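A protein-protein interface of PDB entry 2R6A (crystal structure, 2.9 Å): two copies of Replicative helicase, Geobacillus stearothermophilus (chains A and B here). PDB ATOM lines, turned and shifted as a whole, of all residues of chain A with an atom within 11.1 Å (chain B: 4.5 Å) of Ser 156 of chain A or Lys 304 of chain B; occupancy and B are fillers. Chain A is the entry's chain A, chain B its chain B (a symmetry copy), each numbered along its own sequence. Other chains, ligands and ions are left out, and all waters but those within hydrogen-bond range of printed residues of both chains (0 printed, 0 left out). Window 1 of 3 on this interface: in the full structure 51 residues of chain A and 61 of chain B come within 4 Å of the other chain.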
ATOM      1  N   PRO A  33     -10.615 -20.404  29.602  1.00  0.00           N
ATOM      2  CA  PRO A  33     -10.580 -19.242  28.690  1.00  0.00           C
ATOM      3  C   PRO A  33     -11.743 -19.217  27.717  1.00  0.00           C
ATOM      4  O   PRO A  33     -12.223 -18.140  27.381  1.00  0.00           O
ATOM      5  CB  PRO A  33      -9.290 -19.438  27.896  1.00  0.00           C
ATOM      6  CG  PRO A  33      -8.451 -20.318  28.720  1.00  0.00           C
ATOM      7  CD  PRO A  33      -9.377 -21.202  29.521  1.00  0.00           C
ATOM      8  N   SER A  35     -14.933 -20.508  28.023  1.00  0.00           N
ATOM      9  CA  SER A  35     -16.184 -20.144  28.685  1.00  0.00           C
ATOM     10  C   SER A  35     -16.210 -18.670  29.085  1.00  0.00           C
ATOM     11  O   SER A  35     -17.275 -18.061  29.105  1.00  0.00           O
ATOM     12  CB  SER A  35     -16.420 -21.018  29.900  1.00  0.00           C
ATOM     13  OG  SER A  35     -15.306 -20.907  30.750  1.00  0.00           O
ATOM     14  N   GLU A  36     -15.046 -18.096  29.386  1.00  0.00           N
ATOM     15  CA  GLU A  36     -14.975 -16.674  29.717  1.00  0.00           C
ATOM     16  C   GLU A  36     -15.404 -15.826  28.531  1.00  0.00           C
ATOM     17  O   GLU A  36     -16.173 -14.883  28.692  1.00  0.00           O
ATOM     18  CB  GLU A  36     -13.577 -16.260  30.202  1.00  0.00           C
ATOM     19  CG  GLU A  36     -13.247 -16.745  31.622  1.00  0.00           C
ATOM     20  CD  GLU A  36     -11.886 -16.266  32.139  1.00  0.00           C
ATOM     21  OE1 GLU A  36     -11.257 -15.401  31.478  1.00  0.00           O
ATOM     22  OE2 GLU A  36     -11.456 -16.756  33.216  1.00  0.00           O
ATOM     23  N   ILE A  37     -14.928 -16.187  27.343  1.00  0.00           N
ATOM     24  CA  ILE A  37     -15.209 -15.451  26.109  1.00  0.00           C
ATOM     25  C   ILE A  37     -16.536 -15.830  25.416  1.00  0.00           C
ATOM     26  O   ILE A  37     -17.147 -14.988  24.771  1.00  0.00           O
ATOM     27  CB  ILE A  37     -14.039 -15.633  25.104  1.00  0.00           C
ATOM     28  CG1 ILE A  37     -12.713 -15.202  25.739  1.00  0.00           C
ATOM     29  CG2 ILE A  37     -14.285 -14.865  23.798  1.00  0.00           C
ATOM     30  CD1 ILE A  37     -11.467 -15.625  24.964  1.00  0.00           C
ATOM     31  N   LEU A  38     -16.990 -17.076  25.561  1.00  0.00           N
ATOM     32  CA  LEU A  38     -18.160 -17.557  24.811  1.00  0.00           C
ATOM     33  C   LEU A  38     -19.228 -18.244  25.639  1.00  0.00           C
ATOM     34  O   LEU A  38     -18.925 -18.910  26.621  1.00  0.00           O
ATOM     35  CB  LEU A  38     -17.723 -18.589  23.763  1.00  0.00           C
ATOM     36  CG  LEU A  38     -16.487 -18.337  22.915  1.00  0.00           C
ATOM     37  CD1 LEU A  38     -16.119 -19.593  22.182  1.00  0.00           C
ATOM     38  CD2 LEU A  38     -16.720 -17.194  21.954  1.00  0.00           C
ATOM     39  N   GLU A 103      -7.771 -18.949  23.156  1.00  0.00           N
ATOM     40  CA  GLU A 103      -8.342 -17.600  23.299  1.00  0.00           C
ATOM     41  C   GLU A 103      -8.533 -16.929  21.943  1.00  0.00           C
ATOM     42  O   GLU A 103      -9.560 -16.288  21.690  1.00  0.00           O
ATOM     43  CB  GLU A 103      -7.489 -16.703  24.182  1.00  0.00           C
ATOM     44  CG  GLU A 103      -7.432 -17.128  25.624  1.00  0.00           C
ATOM     45  CD  GLU A 103      -7.151 -15.969  26.566  1.00  0.00           C
ATOM     46  OE1 GLU A 103      -7.352 -14.804  26.138  1.00  0.00           O
ATOM     47  OE2 GLU A 103      -6.747 -16.225  27.728  1.00  0.00           O
ATOM     48  N   ARG A 107     -11.946 -15.812  20.366  1.00  0.00           N
ATOM     49  CA  ARG A 107     -12.248 -14.440  19.993  1.00  0.00           C
ATOM     50  C   ARG A 107     -12.846 -14.363  18.606  1.00  0.00           C
ATOM     51  O   ARG A 107     -13.784 -13.600  18.379  1.00  0.00           O
ATOM     52  CB  ARG A 107     -11.051 -13.518  20.178  1.00  0.00           C
ATOM     53  CG  ARG A 107     -10.929 -13.039  21.612  1.00  0.00           C
ATOM     54  CD  ARG A 107      -9.908 -11.935  21.789  1.00  0.00           C
ATOM     55  NE  ARG A 107      -8.549 -12.459  21.893  1.00  0.00           N
ATOM     56  CZ  ARG A 107      -7.982 -12.841  23.032  1.00  0.00           C
ATOM     57  NH1 ARG A 107      -8.656 -12.764  24.178  1.00  0.00           N
ATOM     58  NH2 ARG A 107      -6.739 -13.308  23.027  1.00  0.00           N
ATOM     59  N   GLU A 110     -16.398 -15.403  18.842  1.00  0.00           N
ATOM     60  CA  GLU A 110     -17.143 -14.317  19.478  1.00  0.00           C
ATOM     61  C   GLU A 110     -17.397 -13.185  18.493  1.00  0.00           C
ATOM     62  O   GLU A 110     -18.527 -12.712  18.374  1.00  0.00           O
ATOM     63  CB  GLU A 110     -16.404 -13.789  20.696  1.00  0.00           C
ATOM     64  CG  GLU A 110     -17.107 -12.655  21.425  1.00  0.00           C
ATOM     65  CD  GLU A 110     -16.128 -11.845  22.239  1.00  0.00           C
ATOM     66  OE1 GLU A 110     -16.246 -11.812  23.485  1.00  0.00           O
ATOM     67  OE2 GLU A 110     -15.203 -11.274  21.625  1.00  0.00           O
ATOM     68  N   VAL A 114     -21.037 -11.558  17.354  1.00  0.00           N
ATOM     69  CA  VAL A 114     -21.389 -10.161  17.543  1.00  0.00           C
ATOM     70  C   VAL A 114     -21.897  -9.565  16.243  1.00  0.00           C
ATOM     71  O   VAL A 114     -22.886  -8.836  16.241  1.00  0.00           O
ATOM     72  CB  VAL A 114     -20.203  -9.351  18.111  1.00  0.00           C
ATOM     73  CG1 VAL A 114     -20.523  -7.872  18.117  1.00  0.00           C
ATOM     74  CG2 VAL A 114     -19.880  -9.830  19.525  1.00  0.00           C
ATOM     75  N   MET A 148     -26.958  -0.078  20.930  1.00  0.00           N
ATOM     76  CA  MET A 148     -25.967  -0.010  22.008  1.00  0.00           C
ATOM     77  C   MET A 148     -25.754  -1.385  22.654  1.00  0.00           C
ATOM     78  O   MET A 148     -24.620  -1.755  22.971  1.00  0.00           O
ATOM     79  CB  MET A 148     -26.366   1.016  23.079  1.00  0.00           C
ATOM     80  CG  MET A 148     -26.715   2.412  22.546  1.00  0.00           C
ATOM     81  SD  MET A 148     -25.384   3.349  21.745  1.00  0.00           S
ATOM     82  CE  MET A 148     -24.462   3.929  23.169  1.00  0.00           C
ATOM     83  N   GLU A 149     -26.849  -2.132  22.821  1.00  0.00           N
ATOM     84  CA  GLU A 149     -26.841  -3.468  23.437  1.00  0.00           C
ATOM     85  C   GLU A 149     -25.941  -4.479  22.736  1.00  0.00           C
ATOM     86  O   GLU A 149     -25.491  -5.448  23.347  1.00  0.00           O
ATOM     87  CB  GLU A 149     -28.262  -4.037  23.523  1.00  0.00           C
ATOM     88  CG  GLU A 149     -29.118  -3.438  24.638  1.00  0.00           C
ATOM     89  CD  GLU A 149     -30.553  -3.981  24.676  1.00  0.00           C
ATOM     90  OE1 GLU A 149     -30.865  -4.980  23.983  1.00  0.00           O
ATOM     91  OE2 GLU A 149     -31.372  -3.395  25.417  1.00  0.00           O
ATOM     92  N   VAL A 150     -25.691  -4.259  21.451  1.00  0.00           N
ATOM     93  CA  VAL A 150     -24.856  -5.168  20.675  1.00  0.00           C
ATOM     94  C   VAL A 150     -23.399  -5.078  21.131  1.00  0.00           C
ATOM     95  O   VAL A 150     -22.732  -6.098  21.292  1.00  0.00           O
ATOM     96  CB  VAL A 150     -24.994  -4.923  19.154  1.00  0.00           C
ATOM     97  CG1 VAL A 150     -24.125  -5.891  18.376  1.00  0.00           C
ATOM     98  CG2 VAL A 150     -26.442  -5.095  18.729  1.00  0.00           C
ATOM     99  N   SER A 151     -22.927  -3.858  21.369  1.00  0.00           N
ATOM    100  CA  SER A 151     -21.554  -3.618  21.803  1.00  0.00           C
ATOM    101  C   SER A 151     -21.302  -4.209  23.188  1.00  0.00           C
ATOM    102  O   SER A 151     -20.348  -4.960  23.376  1.00  0.00           O
ATOM    103  CB  SER A 151     -21.253  -2.119  21.788  1.00  0.00           C
ATOM    104  OG  SER A 151     -19.883  -1.878  22.027  1.00  0.00           O
ATOM    105  N   GLN A 152     -22.166  -3.877  24.147  1.00  0.00           N
ATOM    106  CA  GLN A 152     -22.074  -4.402  25.508  1.00  0.00           C
ATOM    107  C   GLN A 152     -22.487  -5.861  25.505  1.00  0.00           C
ATOM    108  O   GLN A 152     -23.608  -6.207  25.878  1.00  0.00           O
ATOM    109  CB  GLN A 152     -22.946  -3.583  26.470  1.00  0.00           C
ATOM    110  CG  GLN A 152     -22.231  -2.404  27.133  1.00  0.00           C
ATOM    111  CD  GLN A 152     -21.398  -1.582  26.169  1.00  0.00           C
ATOM    112  OE1 GLN A 152     -20.202  -1.402  26.377  1.00  0.00           O
ATOM    113  NE2 GLN A 152     -22.018  -1.102  25.096  1.00  0.00           N
ATOM    114  N   ARG A 153     -21.567  -6.708  25.058  1.00  0.00           N
ATOM    115  CA  ARG A 153     -21.829  -8.124  24.919  1.00  0.00           C
ATOM    116  C   ARG A 153     -20.481  -8.818  24.924  1.00  0.00           C
ATOM    117  O   ARG A 153     -20.289  -9.817  25.621  1.00  0.00           O
ATOM    118  CB  ARG A 153     -22.561  -8.387  23.603  1.00  0.00           C
ATOM    119  CG  ARG A 153     -23.830  -9.189  23.764  1.00  0.00           C
ATOM    120  CD  ARG A 153     -24.696  -9.075  22.523  1.00  0.00           C
ATOM    121  NE  ARG A 153     -26.114  -8.958  22.879  1.00  0.00           N
ATOM    122  CZ  ARG A 153     -27.118  -8.926  22.006  1.00  0.00           C
ATOM    123  NH1 ARG A 153     -26.882  -9.024  20.698  1.00  0.00           N
ATOM    124  NH2 ARG A 153     -28.368  -8.805  22.447  1.00  0.00           N
ATOM    125  N   LYS A 154     -19.551  -8.261  24.146  1.00  0.00           N
ATOM    126  CA  LYS A 154     -18.175  -8.739  24.077  1.00  0.00           C
ATOM    127  C   LYS A 154     -17.554  -8.852  25.469  1.00  0.00           C
ATOM    128  O   LYS A 154     -17.845  -8.037  26.350  1.00  0.00           O
ATOM    129  CB  LYS A 154     -17.331  -7.780  23.241  1.00  0.00           C
ATOM    130  CG  LYS A 154     -17.514  -7.884  21.744  1.00  0.00           C
ATOM    131  CD  LYS A 154     -16.459  -7.038  21.065  1.00  0.00           C
ATOM    132  CE  LYS A 154     -16.140  -7.547  19.679  1.00  0.00           C
ATOM    133  NZ  LYS A 154     -14.903  -6.900  19.165  1.00  0.00           N
ATOM    134  N   HIS A 155     -16.704  -9.861  25.662  1.00  0.00           N
ATOM    135  CA  HIS A 155     -16.031 -10.056  26.944  1.00  0.00           C
ATOM    136  C   HIS A 155     -14.939  -9.011  27.153  1.00  0.00           C
ATOM    137  O   HIS A 155     -13.875  -9.070  26.527  1.00  0.00           O
ATOM    138  CB  HIS A 155     -15.460 -11.471  27.069  1.00  0.00           C
ATOM    139  CG  HIS A 155     -14.552 -11.651  28.246  1.00  0.00           C
ATOM    140  ND1 HIS A 155     -15.024 -11.881  29.520  1.00  0.00           N
ATOM    141  CD2 HIS A 155     -13.202 -11.620  28.345  1.00  0.00           C
ATOM    142  CE1 HIS A 155     -14.002 -11.991  30.352  1.00  0.00           C
ATOM    143  NE2 HIS A 155     -12.885 -11.835  29.663  1.00  0.00           N
ATOM    144  N   SER A 156     -15.222  -8.057  28.035  1.00  0.00           N
ATOM    145  CA  SER A 156     -14.280  -6.998  28.381  1.00  0.00           C
ATOM    146  C   SER A 156     -13.688  -7.257  29.766  1.00  0.00           C
ATOM    147  O   SER A 156     -13.886  -8.328  30.350  1.00  0.00           O
ATOM    148  CB  SER A 156     -14.982  -5.631  28.361  1.00  0.00           C
ATOM    149  OG  SER A 156     -15.523  -5.333  27.086  1.00  0.00           O
ATOM    150  N   GLY A 157     -12.949  -6.272  30.271  1.00  0.00           N
ATOM    151  CA  GLY A 157     -12.387  -6.309  31.619  1.00  0.00           C
ATOM    152  C   GLY A 157     -11.247  -7.288  31.835  1.00  0.00           C
ATOM    153  O   GLY A 157     -10.718  -7.867  30.883  1.00  0.00           O
ATOM    154  N   ALA A 158     -10.847  -7.456  33.095  1.00  0.00           N
ATOM    155  CA  ALA A 158     -11.432  -6.713  34.213  1.00  0.00           C
ATOM    156  C   ALA A 158     -10.504  -5.582  34.653  1.00  0.00           C
ATOM    157  O   ALA A 158      -9.380  -5.462  34.155  1.00  0.00           O
ATOM    158  CB  ALA A 158     -11.715  -7.653  35.380  1.00  0.00           C
ATOM    159  N   PHE A 159     -10.990  -4.736  35.562  1.00  0.00           N
ATOM    160  CA  PHE A 159     -10.157  -3.715  36.188  1.00  0.00           C
ATOM    161  C   PHE A 159      -9.192  -4.419  37.130  1.00  0.00           C
ATOM    162  O   PHE A 159      -9.606  -5.302  37.897  1.00  0.00           O
ATOM    163  CB  PHE A 159     -10.995  -2.779  37.062  1.00  0.00           C
ATOM    164  CG  PHE A 159     -11.808  -1.769  36.310  1.00  0.00           C
ATOM    165  CD1 PHE A 159     -11.217  -0.608  35.815  1.00  0.00           C
ATOM    166  CD2 PHE A 159     -13.183  -1.940  36.163  1.00  0.00           C
ATOM    167  CE1 PHE A 159     -11.975   0.344  35.149  1.00  0.00           C
ATOM    168  CE2 PHE A 159     -13.952  -0.991  35.498  1.00  0.00           C
ATOM    169  CZ  PHE A 159     -13.348   0.152  34.989  1.00  0.00           C
ATOM    170  N   LYS A 160      -7.916  -4.053  37.086  1.00  0.00           N
ATOM    171  CA  LYS A 160      -6.999  -4.556  38.107  1.00  0.00           C
ATOM    172  C   LYS A 160      -7.209  -3.745  39.392  1.00  0.00           C
ATOM    173  O   LYS A 160      -7.205  -2.509  39.363  1.00  0.00           O
ATOM    174  CB  LYS A 160      -5.527  -4.543  37.668  1.00  0.00           C
ATOM    175  CG  LYS A 160      -5.058  -3.304  36.922  1.00  0.00           C
ATOM    176  CD  LYS A 160      -4.685  -3.615  35.480  1.00  0.00           C
ATOM    177  CE  LYS A 160      -3.429  -4.480  35.416  1.00  0.00           C
ATOM    178  NZ  LYS A 160      -2.778  -4.453  34.082  1.00  0.00           N
ATOM    179  N   ASP B 291      -7.584   0.722  34.891  1.00  0.00           N
ATOM    180  CA  ASP B 291      -7.521   0.083  33.586  1.00  0.00           C
ATOM    181  C   ASP B 291      -6.489   0.849  32.752  1.00  0.00           C
ATOM    182  O   ASP B 291      -6.717   2.003  32.373  1.00  0.00           O
ATOM    183  CB  ASP B 291      -8.899   0.095  32.922  1.00  0.00           C
ATOM    184  CG  ASP B 291      -8.906  -0.570  31.559  1.00  0.00           C
ATOM    185  OD1 ASP B 291      -7.872  -1.130  31.131  1.00  0.00           O
ATOM    186  OD2 ASP B 291      -9.961  -0.529  30.903  1.00  0.00           O
ATOM    187  N   THR B 293      -5.142  -0.175  29.709  1.00  0.00           N
ATOM    188  CA  THR B 293      -5.093  -0.688  28.341  1.00  0.00           C
ATOM    189  C   THR B 293      -4.943   0.484  27.352  1.00  0.00           C
ATOM    190  O   THR B 293      -5.814   1.355  27.293  1.00  0.00           O
ATOM    191  CB  THR B 293      -6.326  -1.578  28.001  1.00  0.00           C
ATOM    192  OG1 THR B 293      -7.510  -0.990  28.549  1.00  0.00           O
ATOM    193  CG2 THR B 293      -6.171  -2.982  28.589  1.00  0.00           C
ATOM    194  N   ILE B 296      -8.271   2.533  24.220  1.00  0.00           N
ATOM    195  CA  ILE B 296      -9.572   2.023  24.634  1.00  0.00           C
ATOM    196  C   ILE B 296     -10.695   2.769  23.901  1.00  0.00           C
ATOM    197  O   ILE B 296     -10.531   3.930  23.512  1.00  0.00           O
ATOM    198  CB  ILE B 296      -9.739   2.125  26.175  1.00  0.00           C
ATOM    199  CG1 ILE B 296     -10.911   1.257  26.655  1.00  0.00           C
ATOM    200  CG2 ILE B 296      -9.857   3.590  26.618  1.00  0.00           C
ATOM    201  CD1 ILE B 296     -11.009   1.081  28.165  1.00  0.00           C
ATOM    202  N   ASP B 300     -16.008   0.260  25.474  1.00  0.00           N
ATOM    203  CA  ASP B 300     -15.230  -0.635  26.346  1.00  0.00           C
ATOM    204  C   ASP B 300     -15.190  -0.066  27.766  1.00  0.00           C
ATOM    205  O   ASP B 300     -15.125  -0.811  28.752  1.00  0.00           O
ATOM    206  CB  ASP B 300     -13.796  -0.814  25.836  1.00  0.00           C
ATOM    207  CG  ASP B 300     -13.728  -1.248  24.384  1.00  0.00           C
ATOM    208  OD1 ASP B 300     -14.737  -1.757  23.835  1.00  0.00           O
ATOM    209  OD2 ASP B 300     -12.644  -1.075  23.790  1.00  0.00           O
ATOM    210  N   ILE B 301     -15.214   1.263  27.855  1.00  0.00           N
ATOM    211  CA  ILE B 301     -15.296   1.949  29.132  1.00  0.00           C
ATOM    212  C   ILE B 301     -16.633   1.576  29.777  1.00  0.00           C
ATOM    213  O   ILE B 301     -16.666   1.155  30.936  1.00  0.00           O
ATOM    214  CB  ILE B 301     -15.155   3.490  28.967  1.00  0.00           C
ATOM    215  CG1 ILE B 301     -13.812   3.835  28.307  1.00  0.00           C
ATOM    216  CG2 ILE B 301     -15.308   4.196  30.313  1.00  0.00           C
ATOM    217  CD1 ILE B 301     -13.599   5.310  28.002  1.00  0.00           C
ATOM    218  N   ARG B 302     -17.715   1.684  29.005  1.00  0.00           N
ATOM    219  CA  ARG B 302     -19.063   1.396  29.505  1.00  0.00           C
ATOM    220  C   ARG B 302     -19.218  -0.029  30.013  1.00  0.00           C
ATOM    221  O   ARG B 302     -19.759  -0.239  31.095  1.00  0.00           O
ATOM    222  CB  ARG B 302     -20.137   1.661  28.447  1.00  0.00           C
ATOM    223  CG  ARG B 302     -19.968   2.934  27.646  1.00  0.00           C
ATOM    224  CD  ARG B 302     -21.314   3.555  27.264  1.00  0.00           C
ATOM    225  NE  ARG B 302     -22.376   2.575  27.035  1.00  0.00           N
ATOM    226  CZ  ARG B 302     -22.579   1.925  25.894  1.00  0.00           C
ATOM    227  NH1 ARG B 302     -21.780   2.117  24.847  1.00  0.00           N
ATOM    228  NH2 ARG B 302     -23.585   1.065  25.802  1.00  0.00           N
ATOM    229  N   ALA B 303     -18.748  -0.997  29.227  1.00  0.00           N
ATOM    230  CA  ALA B 303     -18.849  -2.416  29.583  1.00  0.00           C
ATOM    231  C   ALA B 303     -18.219  -2.698  30.944  1.00  0.00           C
ATOM    232  O   ALA B 303     -18.843  -3.313  31.812  1.00  0.00           O
ATOM    233  CB  ALA B 303     -18.210  -3.293  28.501  1.00  0.00           C
ATOM    234  N   LYS B 304     -16.991  -2.223  31.122  1.00  0.00           N
ATOM    235  CA  LYS B 304     -16.251  -2.416  32.363  1.00  0.00           C
ATOM    236  C   LYS B 304     -16.861  -1.644  33.534  1.00  0.00           C
ATOM    237  O   LYS B 304     -16.873  -2.136  34.664  1.00  0.00           O
ATOM    238  CB  LYS B 304     -14.777  -2.051  32.170  1.00  0.00           C
ATOM    239  CG  LYS B 304     -14.060  -2.928  31.152  1.00  0.00           C
ATOM    240  CD  LYS B 304     -12.655  -2.435  30.872  1.00  0.00           C
ATOM    241  CE  LYS B 304     -12.065  -3.139  29.660  1.00  0.00           C
ATOM    242  NZ  LYS B 304     -10.754  -2.569  29.275  1.00  0.00           N
ATOM    243  N   CYS B 305     -17.373  -0.445  33.259  1.00  0.00           N
ATOM    244  CA  CYS B 305     -18.011   0.380  34.292  1.00  0.00           C
ATOM    245  C   CYS B 305     -19.393  -0.145  34.716  1.00  0.00           C
ATOM    246  O   CYS B 305     -19.733  -0.107  35.898  1.00  0.00           O
ATOM    247  CB  CYS B 305     -18.087   1.850  33.857  1.00  0.00           C
ATOM    248  SG  CYS B 305     -16.492   2.712  33.829  1.00  0.00           S
ATOM    249  N   ARG B 306     -20.179  -0.623  33.753  1.00  0.00           N
ATOM    250  CA  ARG B 306     -21.488  -1.204  34.052  1.00  0.00           C
ATOM    251  C   ARG B 306     -21.338  -2.483  34.878  1.00  0.00           C
ATOM    252  O   ARG B 306     -22.065  -2.678  35.856  1.00  0.00           O
ATOM    253  CB  ARG B 306     -22.294  -1.464  32.770  1.00  0.00           C
ATOM    254  CG  ARG B 306     -22.887  -0.206  32.140  1.00  0.00           C
ATOM    255  CD  ARG B 306     -23.393  -0.425  30.711  1.00  0.00           C
ATOM    256  NE  ARG B 306     -24.559  -1.307  30.633  1.00  0.00           N
ATOM    257  CZ  ARG B 306     -24.516  -2.592  30.288  1.00  0.00           C
ATOM    258  NH1 ARG B 306     -23.365  -3.175  29.982  1.00  0.00           N
ATOM    259  NH2 ARG B 306     -25.636  -3.300  30.249  1.00  0.00           N
ATOM    260  N   ARG B 307     -20.388  -3.339  34.491  1.00  0.00           N
ATOM    261  CA  ARG B 307     -20.120  -4.591  35.209  1.00  0.00           C
ATOM    262  C   ARG B 307     -19.543  -4.329  36.598  1.00  0.00           C
ATOM    263  O   ARG B 307     -19.705  -5.152  37.498  1.00  0.00           O
ATOM    264  CB  ARG B 307     -19.180  -5.519  34.421  1.00  0.00           C
ATOM    265  CG  ARG B 307     -19.777  -6.132  33.148  1.00  0.00           C
ATOM    266  CD  ARG B 307     -18.802  -7.134  32.510  1.00  0.00           C
ATOM    267  NE  ARG B 307     -19.211  -7.543  31.162  1.00  0.00           N
ATOM    268  CZ  ARG B 307     -18.608  -8.481  30.428  1.00  0.00           C
ATOM    269  NH1 ARG B 307     -17.556  -9.142  30.894  1.00  0.00           N
ATOM    270  NH2 ARG B 307     -19.066  -8.765  29.217  1.00  0.00           N
ATOM    271  N   LEU B 308     -18.874  -3.187  36.767  1.00  0.00           N
ATOM    272  CA  LEU B 308     -18.304  -2.807  38.060  1.00  0.00           C
ATOM    273  C   LEU B 308     -19.382  -2.316  39.030  1.00  0.00           C
ATOM    274  O   LEU B 308     -19.436  -2.768  40.176  1.00  0.00           O
ATOM    275  CB  LEU B 308     -17.205  -1.748  37.900  1.00  0.00           C
ATOM    276  CG  LEU B 308     -16.562  -1.203  39.188  1.00  0.00           C
ATOM    277  CD1 LEU B 308     -15.800  -2.283  39.964  1.00  0.00           C
ATOM    278  CD2 LEU B 308     -15.666  -0.007  38.893  1.00  0.00           C
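Hydrophobic or aromatic side chains of chain B within 4 Å of the printed part of chain A: Ala 303 and Leu 308. Along chain B the printed residues that touch a printed residue of chain A span positions 291 to 308. Among the printed residues, 14 pairs touch across the chains. Among the printed residues, no Asp or Glu carboxylate lies within 4 Å of a Lys or Arg side-chain nitrogen of the other chain.
A ring nitrogen (ND1) of His 155 of chain A sits at hydrogen-bond distance from the backbone carbonyl oxygen (O) of Glu 36 of chain A (3.3 Å). The side-chain carboxylate of Glu 110 of chain A is in hydrogen-bond range of the backbone NH of His 155 of chain A, 3.0 Å away. O of Met 148 of chain A is in hydrogen-bond range of NE2 of Gln 152 of chain A, 3.4 Å away. The side-chain amino group (NZ) of Lys 304 of chain B lies within salt-bridge range of the side-chain carboxylate (OD2) of Asp 291 of chain B, at 2.7 Å. The side-chain hydroxyl of Thr 293 of chain B is in hydrogen-bond range of the side-chain carboxylate of Asp 291 of chain B, 2.6 Å away.
Of the printed residues of chain B, Ser 156 of chain A touches Ala 303, Lys 304 and Arg 307. Of the printed residues of chain A, Lys 304 of chain B touches Ser 156 (3.99 Å), Gly 157 (3.3 Å) and Phe 159 (3.2 Å). Cys 305 of chain B touches none of the printed residues of chain A. Of chain A, only Arg 153, Lys 154, His 155 and Ser 156 come within 4 Å of Arg 307 of chain B. Of chain A, only Phe 159 comes within 4 Å of Leu 308 of chain B. Printed residues of chain B within 4 Å of Gln 152 of chain A: Arg 302 (2.8 Å), Ala 303 (3.2 Å) and Arg 306 (3.2 Å). Printed residues of chain B within 4 Å of His 155 of chain A: Arg 307 (3.98 Å). Of the printed residues of chain A, Asp 291 of chain B touches Phe 159 (3.8 Å). Printed residues of chain A within 4 Å of Arg 306 of chain B: Gln 152 (3.2 Å). Printed residues of chain B within 4 Å of Phe 159 of chain A: Asp 291 (3.8 Å), Lys 304 (3.2 Å) and Leu 308 (3.9 Å). Ser 151 of chain A touches none of the printed residues of chain B. Val 114 of chain A touches none of the printed residues of chain B. The nearest printed residue of chain B that does not touch Ser 156 of chain A is Asp 300 of chain B (4.8 Å).
No position is printed for both chains. Of the 14 pairs that touch across the chains among the printed residues, none has its exchanged pair printed and touching as well.
OE1 of Gln 152 of chain A is in hydrogen-bond range of N of Ala 303 of chain B (3.2 Å). The guanidinium group of Arg 307 of chain B is in hydrogen-bond range of the backbone carbonyl oxygen of Lys 154 of chain A, at 3.2 Å. The guanidinium group (NH2) of Arg 302 of chain B lies close to the side-chain amide nitrogen (NE2) of Gln 152 of chain A, 2.8 Å away.
CE of Met 148 of chain A touches NH1 of Arg 302 of chain B, at 3.6 Å. Arg 306 of chain B touches Gln 152 of chain A. Arg 153 of chain A touches Arg 307 of chain B (O to NH2, 3.9 Å). His 155 of chain A touches Arg 307 of chain B. Ser 156 of chain A touches Ala 303 of chain B. CG of Lys 304 of chain B touches CB of Ser 156 of chain A, at 3.99 Å. Arg 307 of chain B touches Ser 156 of chain A (NH1 to O, 3.8 Å). Asp 291 of chain B touches Phe 159 of chain A. Lys 304 of chain B touches Phe 159 of chain A (O to CE2, 3.2 Å). Phe 159 of chain A touches Leu 308 of chain B.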
